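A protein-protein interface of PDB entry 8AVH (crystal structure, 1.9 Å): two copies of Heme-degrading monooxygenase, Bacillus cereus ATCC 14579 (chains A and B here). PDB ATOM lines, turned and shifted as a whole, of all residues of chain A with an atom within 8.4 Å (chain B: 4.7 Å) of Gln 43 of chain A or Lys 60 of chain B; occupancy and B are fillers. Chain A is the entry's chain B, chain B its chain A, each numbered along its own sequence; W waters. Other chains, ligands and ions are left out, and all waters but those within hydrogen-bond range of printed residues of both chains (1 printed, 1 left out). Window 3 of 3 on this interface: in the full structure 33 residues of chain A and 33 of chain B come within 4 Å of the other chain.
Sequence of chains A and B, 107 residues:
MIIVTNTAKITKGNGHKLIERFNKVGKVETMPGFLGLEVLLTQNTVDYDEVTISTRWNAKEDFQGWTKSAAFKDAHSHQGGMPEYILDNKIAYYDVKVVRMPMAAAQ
The side-chain amino group (NZ) of Lys 60 of chain B is in hydrogen-bond range of the side-chain amide oxygen (OE1) of Gln 43 of chain A, 2.7 Å away.
N of Gln 43 of chain A sits at hydrogen-bond distance from O of Tyr 93 of chain B, at 2.8 Å.
The backbone NH (N) of Asp 95 of chain B sits at hydrogen-bond distance from the backbone carbonyl oxygen (O) of Leu 41 of chain A.
The side-chain amide nitrogen (NE2) of Gln 43 of chain A is in hydrogen-bond range of the side-chain carboxylate (OD1) of Asp 95 of chain B (3.0 Å).
OG1 of Thr 42 of chain A lies within hydrogen-bond range of OE1 of Glu 50 of chain A, 2.7 Å away.
Asp 95 of chain B touches Leu 40 of chain A.
Tyr 94 of chain B touches Leu 41 of chain A (CA to O, 3.6 Å).
Thr 42 of chain A touches Tyr 93 of chain B.
Thr 42 of chain A touches Tyr 94 of chain B.
Printed residues of chain B within 4 Å of Leu 40 of chain A: Asp 95.
Printed residues of chain B within 4 Å of Thr 42 of chain A: Tyr 93 (3.6 Å) and Tyr 94 (3.2 Å).
No residue of chain A comes within 4 Å of Ala 59 of chain B.
Of chain A, only Gln 43 comes within 4 Å of Lys 60 of chain B.
Printed residues of chain A within 4 Å of Asp 95 of chain B: Leu 40 (3.3 Å), Leu 41 (3.0 Å) and Gln 43 (3.0 Å).
The nearest residue of chain A that does not touch Lys 60 of chain B is Asn 44 of chain A (5.1 Å).
Of the 10 printed residues of chain B, 4 touch a printed residue of chain A.
Printed residues of chain A that touch a printed residue of chain B: Leu 40, Leu 41, Thr 42 and Gln 43.
Hydrophobic or aromatic side chains of chain A within 4 Å of the printed part of chain B: Leu 40.
Among the printed residues, 8 pairs touch across the chains.
No position is printed for both chains.
Of the 8 pairs that touch across the chains among the printed residues, none has its exchanged pair printed and touching as well.
Water W1 lies within hydrogen-bond range of N of Tyr 93 of chain B (2.8 Å) and O of Gln 43 of chain A (2.9 Å).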
ATOM      1  N   LYS A  12      41.658 -18.400  -1.958  1.00  0.00           N
ATOM      2  CA  LYS A  12      40.350 -17.972  -1.476  1.00  0.00           C
ATOM      3  C   LYS A  12      39.930 -16.684  -2.161  1.00  0.00           C
ATOM      4  O   LYS A  12      40.697 -15.721  -2.221  1.00  0.00           O
ATOM      5  CB  LYS A  12      40.382 -17.772   0.042  1.00  0.00           C
ATOM      6  CG  LYS A  12      39.035 -17.453   0.659  1.00  0.00           C
ATOM      7  CD  LYS A  12      38.226 -18.721   0.884  1.00  0.00           C
ATOM      8  CE  LYS A  12      36.978 -18.445   1.727  1.00  0.00           C
ATOM      9  NZ  LYS A  12      36.161 -19.678   1.905  1.00  0.00           N
ATOM     10  N   LEU A  40      31.374 -27.966  -8.879  1.00  0.00           N
ATOM     11  CA  LEU A  40      30.963 -27.809  -7.495  1.00  0.00           C
ATOM     12  C   LEU A  40      31.912 -26.858  -6.778  1.00  0.00           C
ATOM     13  O   LEU A  40      33.109 -26.809  -7.074  1.00  0.00           O
ATOM     14  CB  LEU A  40      30.989 -29.147  -6.754  1.00  0.00           C
ATOM     15  CG  LEU A  40      30.415 -30.350  -7.509  1.00  0.00           C
ATOM     16  CD1 LEU A  40      30.666 -31.629  -6.715  1.00  0.00           C
ATOM     17  CD2 LEU A  40      28.936 -30.151  -7.713  1.00  0.00           C
ATOM     18  N   LEU A  41      31.368 -26.135  -5.810  1.00  0.00           N
ATOM     19  CA  LEU A  41      32.135 -25.272  -4.921  1.00  0.00           C
ATOM     20  C   LEU A  41      31.896 -25.749  -3.501  1.00  0.00           C
ATOM     21  O   LEU A  41      30.752 -25.757  -3.038  1.00  0.00           O
ATOM     22  CB  LEU A  41      31.700 -23.814  -5.085  1.00  0.00           C
ATOM     23  CG  LEU A  41      32.413 -22.794  -4.183  1.00  0.00           C
ATOM     24  CD1 LEU A  41      33.879 -22.726  -4.542  1.00  0.00           C
ATOM     25  CD2 LEU A  41      31.767 -21.439  -4.323  1.00  0.00           C
ATOM     26  N   THR A  42      32.956 -26.183  -2.825  1.00  0.00           N
ATOM     27  CA  THR A  42      32.800 -26.713  -1.477  1.00  0.00           C
ATOM     28  C   THR A  42      32.369 -25.589  -0.534  1.00  0.00           C
ATOM     29  O   THR A  42      32.875 -24.470  -0.618  1.00  0.00           O
ATOM     30  CB  THR A  42      34.109 -27.358  -1.007  1.00  0.00           C
ATOM     31  OG1 THR A  42      34.556 -28.311  -1.980  1.00  0.00           O
ATOM     32  CG2 THR A  42      33.928 -28.096   0.324  1.00  0.00           C
ATOM     33  N   GLN A  43      31.394 -25.876   0.337  1.00  0.00           N
ATOM     34  CA  GLN A  43      30.976 -24.906   1.344  1.00  0.00           C
ATOM     35  C   GLN A  43      31.935 -24.897   2.531  1.00  0.00           C
ATOM     36  O   GLN A  43      32.567 -25.903   2.855  1.00  0.00           O
ATOM     37  CB  GLN A  43      29.562 -25.208   1.846  1.00  0.00           C
ATOM     38  CG  GLN A  43      28.470 -24.993   0.810  1.00  0.00           C
ATOM     39  CD  GLN A  43      27.087 -25.145   1.408  1.00  0.00           C
ATOM     40  OE1 GLN A  43      26.946 -25.453   2.590  1.00  0.00           O
ATOM     41  NE2 GLN A  43      26.061 -24.933   0.598  1.00  0.00           N
ATOM     42  N   ASN A  44      32.038 -23.737   3.183  1.00  0.00           N
ATOM     43  CA  ASN A  44      32.741 -23.616   4.464  1.00  0.00           C
ATOM     44  C   ASN A  44      34.187 -24.093   4.387  1.00  0.00           C
ATOM     45  O   ASN A  44      34.656 -24.830   5.253  1.00  0.00           O
ATOM     46  CB  ASN A  44      32.018 -24.384   5.573  1.00  0.00           C
ATOM     47  CG  ASN A  44      30.523 -24.442   5.364  1.00  0.00           C
ATOM     48  OD1 ASN A  44      29.908 -23.476   4.899  1.00  0.00           O
ATOM     49  ND2 ASN A  44      29.926 -25.586   5.697  1.00  0.00           N
ATOM     50  N   THR A  45      34.897 -23.710   3.336  1.00  0.00           N
ATOM     51  CA  THR A  45      36.342 -23.857   3.332  1.00  0.00           C
ATOM     52  C   THR A  45      36.922 -22.516   3.747  1.00  0.00           C
ATOM     53  O   THR A  45      36.545 -21.478   3.195  1.00  0.00           O
ATOM     54  CB  THR A  45      36.876 -24.276   1.962  1.00  0.00           C
ATOM     55  OG1 THR A  45      36.312 -23.416   0.970  1.00  0.00           O
ATOM     56  CG2 THR A  45      36.518 -25.738   1.663  1.00  0.00           C
ATOM     57  N   VAL A  46      37.808 -22.537   4.737  1.00  0.00           N
ATOM     58  CA  VAL A  46      38.194 -21.298   5.403  1.00  0.00           C
ATOM     59  C   VAL A  46      39.294 -20.579   4.627  1.00  0.00           C
ATOM     60  O   VAL A  46      39.145 -19.415   4.240  1.00  0.00           O
ATOM     61  CB  VAL A  46      38.617 -21.578   6.858  1.00  0.00           C
ATOM     62  CG1 VAL A  46      38.613 -20.286   7.670  1.00  0.00           C
ATOM     63  CG2 VAL A  46      37.698 -22.618   7.494  1.00  0.00           C
ATOM     64  N   TYR A  48      40.817 -21.328   1.667  1.00  0.00           N
ATOM     65  CA  TYR A  48      40.944 -21.496   0.229  1.00  0.00           C
ATOM     66  C   TYR A  48      39.569 -21.796  -0.343  1.00  0.00           C
ATOM     67  O   TYR A  48      38.629 -22.102   0.390  1.00  0.00           O
ATOM     68  CB  TYR A  48      41.930 -22.614  -0.108  1.00  0.00           C
ATOM     69  CG  TYR A  48      41.569 -23.950   0.514  1.00  0.00           C
ATOM     70  CD1 TYR A  48      42.042 -24.306   1.771  1.00  0.00           C
ATOM     71  CD2 TYR A  48      40.744 -24.850  -0.153  1.00  0.00           C
ATOM     72  CE1 TYR A  48      41.709 -25.526   2.343  1.00  0.00           C
ATOM     73  CE2 TYR A  48      40.401 -26.069   0.414  1.00  0.00           C
ATOM     74  CZ  TYR A  48      40.889 -26.402   1.659  1.00  0.00           C
ATOM     75  OH  TYR A  48      40.562 -27.613   2.223  1.00  0.00           O
ATOM     76  N   ASP A  49      39.456 -21.658  -1.658  1.00  0.00           N
ATOM     77  CA  ASP A  49      38.294 -22.156  -2.376  1.00  0.00           C
ATOM     78  C   ASP A  49      38.610 -23.549  -2.897  1.00  0.00           C
ATOM     79  O   ASP A  49      39.760 -23.867  -3.207  1.00  0.00           O
ATOM     80  CB  ASP A  49      37.930 -21.240  -3.544  1.00  0.00           C
ATOM     81  CG  ASP A  49      37.302 -19.941  -3.098  1.00  0.00           C
ATOM     82  OD1 ASP A  49      36.636 -19.937  -2.042  1.00  0.00           O
ATOM     83  OD2 ASP A  49      37.463 -18.924  -3.807  1.00  0.00           O
ATOM     84  N   GLU A  50      37.587 -24.388  -3.000  1.00  0.00           N
ATOM     85  CA  GLU A  50      37.782 -25.723  -3.543  1.00  0.00           C
ATOM     86  C   GLU A  50      36.742 -25.946  -4.628  1.00  0.00           C
ATOM     87  O   GLU A  50      35.538 -25.894  -4.363  1.00  0.00           O
ATOM     88  CB  GLU A  50      37.696 -26.783  -2.447  1.00  0.00           C
ATOM     89  CG  GLU A  50      37.917 -28.183  -2.970  1.00  0.00           C
ATOM     90  CD  GLU A  50      37.911 -29.225  -1.864  1.00  0.00           C
ATOM     91  OE1 GLU A  50      36.829 -29.486  -1.275  1.00  0.00           O
ATOM     92  OE2 GLU A  50      39.000 -29.766  -1.572  1.00  0.00           O
ATOM     93  N   ILE B   2      22.265 -28.570  -4.084  1.00  0.00           N
ATOM     94  CA  ILE B   2      23.425 -28.901  -3.266  1.00  0.00           C
ATOM     95  C   ILE B   2      23.655 -30.410  -3.273  1.00  0.00           C
ATOM     96  O   ILE B   2      22.762 -31.204  -3.571  1.00  0.00           O
ATOM     97  CB  ILE B   2      23.305 -28.396  -1.814  1.00  0.00           C
ATOM     98  CG1 ILE B   2      22.138 -29.051  -1.102  1.00  0.00           C
ATOM     99  CG2 ILE B   2      23.164 -26.864  -1.771  1.00  0.00           C
ATOM    100  CD1 ILE B   2      22.420 -29.314   0.334  1.00  0.00           C
ATOM    101  N   ALA B  59      17.725 -27.833  -2.362  1.00  0.00           N
ATOM    102  CA  ALA B  59      18.257 -26.781  -1.502  1.00  0.00           C
ATOM    103  C   ALA B  59      18.681 -27.379  -0.169  1.00  0.00           C
ATOM    104  O   ALA B  59      18.220 -28.456   0.225  1.00  0.00           O
ATOM    105  CB  ALA B  59      17.229 -25.666  -1.275  1.00  0.00           C
ATOM    106  N   LYS B  60      19.548 -26.652   0.541  1.00  0.00           N
ATOM    107  CA  LYS B  60      20.016 -27.163   1.822  1.00  0.00           C
ATOM    108  C   LYS B  60      18.875 -27.343   2.818  1.00  0.00           C
ATOM    109  O   LYS B  60      18.908 -28.272   3.629  1.00  0.00           O
ATOM    110  CB  LYS B  60      21.095 -26.264   2.421  1.00  0.00           C
ATOM    111  CG  LYS B  60      21.595 -26.810   3.754  1.00  0.00           C
ATOM    112  CD  LYS B  60      22.619 -25.916   4.399  1.00  0.00           C
ATOM    113  CE  LYS B  60      23.929 -25.991   3.666  1.00  0.00           C
ATOM    114  NZ  LYS B  60      24.991 -25.330   4.456  1.00  0.00           N
ATOM    115  N   GLU B  61      17.843 -26.504   2.766  1.00  0.00           N
ATOM    116  CA  GLU B  61      16.783 -26.686   3.755  1.00  0.00           C
ATOM    117  C   GLU B  61      16.035 -27.998   3.537  1.00  0.00           C
ATOM    118  O   GLU B  61      15.497 -28.559   4.497  1.00  0.00           O
ATOM    119  CB  GLU B  61      15.818 -25.491   3.753  1.00  0.00           C
ATOM    120  CG  GLU B  61      15.039 -25.257   2.489  1.00  0.00           C
ATOM    121  CD  GLU B  61      14.040 -24.100   2.638  1.00  0.00           C
ATOM    122  OE1 GLU B  61      14.322 -23.152   3.407  1.00  0.00           O
ATOM    123  OE2 GLU B  61      12.967 -24.146   1.996  1.00  0.00           O
ATOM    124  N   ASP B  62      16.039 -28.524   2.311  1.00  0.00           N
ATOM    125  CA  ASP B  62      15.460 -29.842   2.073  1.00  0.00           C
ATOM    126  C   ASP B  62      16.255 -30.939   2.780  1.00  0.00           C
ATOM    127  O   ASP B  62      15.663 -31.852   3.375  1.00  0.00           O
ATOM    128  CB  ASP B  62      15.380 -30.119   0.579  1.00  0.00           C
ATOM    129  CG  ASP B  62      14.566 -29.069  -0.158  1.00  0.00           C
ATOM    130  OD1 ASP B  62      13.506 -28.649   0.360  1.00  0.00           O
ATOM    131  OD2 ASP B  62      15.004 -28.659  -1.248  1.00  0.00           O
ATOM    132  N   PHE B  63      17.588 -30.880   2.710  1.00  0.00           N
ATOM    133  CA  PHE B  63      18.415 -31.818   3.461  1.00  0.00           C
ATOM    134  C   PHE B  63      18.181 -31.673   4.955  1.00  0.00           C
ATOM    135  O   PHE B  63      18.095 -32.665   5.690  1.00  0.00           O
ATOM    136  CB  PHE B  63      19.885 -31.580   3.145  1.00  0.00           C
ATOM    137  CG  PHE B  63      20.838 -32.336   4.030  1.00  0.00           C
ATOM    138  CD1 PHE B  63      21.026 -33.711   3.865  1.00  0.00           C
ATOM    139  CD2 PHE B  63      21.577 -31.679   4.997  1.00  0.00           C
ATOM    140  CE1 PHE B  63      21.907 -34.404   4.679  1.00  0.00           C
ATOM    141  CE2 PHE B  63      22.467 -32.368   5.805  1.00  0.00           C
ATOM    142  CZ  PHE B  63      22.642 -33.739   5.633  1.00  0.00           C
ATOM    143  N   GLN B  64      18.091 -30.435   5.421  1.00  0.00           N
ATOM    144  CA  GLN B  64      17.921 -30.204   6.847  1.00  0.00           C
ATOM    145  C   GLN B  64      16.598 -30.771   7.324  1.00  0.00           C
ATOM    146  O   GLN B  64      16.518 -31.334   8.419  1.00  0.00           O
ATOM    147  CB  GLN B  64      18.028 -28.707   7.137  1.00  0.00           C
ATOM    148  CG  GLN B  64      19.464 -28.261   7.271  1.00  0.00           C
ATOM    149  CD  GLN B  64      19.596 -26.753   7.302  1.00  0.00           C
ATOM    150  OE1 GLN B  64      18.656 -26.031   6.974  1.00  0.00           O
ATOM    151  NE2 GLN B  64      20.772 -26.270   7.676  1.00  0.00           N
ATOM    152  N   TYR B  93      29.712 -30.357   2.228  1.00  0.00           N
ATOM    153  CA  TYR B  93      28.590 -29.770   1.514  1.00  0.00           C
ATOM    154  C   TYR B  93      29.121 -29.067   0.277  1.00  0.00           C
ATOM    155  O   TYR B  93      30.154 -28.403   0.335  1.00  0.00           O
ATOM    156  CB  TYR B  93      27.823 -28.748   2.388  1.00  0.00           C
ATOM    157  CG  TYR B  93      27.260 -29.336   3.662  1.00  0.00           C
ATOM    158  CD1 TYR B  93      25.997 -29.907   3.687  1.00  0.00           C
ATOM    159  CD2 TYR B  93      28.001 -29.344   4.832  1.00  0.00           C
ATOM    160  CE1 TYR B  93      25.480 -30.450   4.849  1.00  0.00           C
ATOM    161  CE2 TYR B  93      27.491 -29.892   5.996  1.00  0.00           C
ATOM    162  CZ  TYR B  93      26.232 -30.437   5.993  1.00  0.00           C
ATOM    163  OH  TYR B  93      25.712 -30.974   7.145  1.00  0.00           O
ATOM    164  N   TYR B  94      28.400 -29.183  -0.829  1.00  0.00           N
ATOM    165  CA  TYR B  94      28.819 -28.607  -2.098  1.00  0.00           C
ATOM    166  C   TYR B  94      27.656 -27.868  -2.721  1.00  0.00           C
ATOM    167  O   TYR B  94      26.535 -28.392  -2.763  1.00  0.00           O
ATOM    168  CB  TYR B  94      29.296 -29.679  -3.093  1.00  0.00           C
ATOM    169  CG  TYR B  94      30.459 -30.519  -2.623  1.00  0.00           C
ATOM    170  CD1 TYR B  94      30.242 -31.674  -1.884  1.00  0.00           C
ATOM    171  CD2 TYR B  94      31.771 -30.176  -2.937  1.00  0.00           C
ATOM    172  CE1 TYR B  94      31.280 -32.456  -1.465  1.00  0.00           C
ATOM    173  CE2 TYR B  94      32.832 -30.958  -2.512  1.00  0.00           C
ATOM    174  CZ  TYR B  94      32.570 -32.101  -1.775  1.00  0.00           C
ATOM    175  OH  TYR B  94      33.576 -32.911  -1.326  1.00  0.00           O
ATOM    176  N   ASP B  95      27.929 -26.672  -3.232  1.00  0.00           N
ATOM    177  CA  ASP B  95      27.007 -25.967  -4.111  1.00  0.00           C
ATOM    178  C   ASP B  95      27.260 -26.405  -5.547  1.00  0.00           C
ATOM    179  O   ASP B  95      28.410 -26.374  -6.002  1.00  0.00           O
ATOM    180  CB  ASP B  95      27.218 -24.450  -4.017  1.00  0.00           C
ATOM    181  CG  ASP B  95      26.728 -23.864  -2.699  1.00  0.00           C
ATOM    182  OD1 ASP B  95      25.610 -24.213  -2.268  1.00  0.00           O
ATOM    183  OD2 ASP B  95      27.466 -23.056  -2.104  1.00  0.00           O
HETATM  184  O   HOH W   1      31.721 -28.657   3.299  1.00  0.00           O
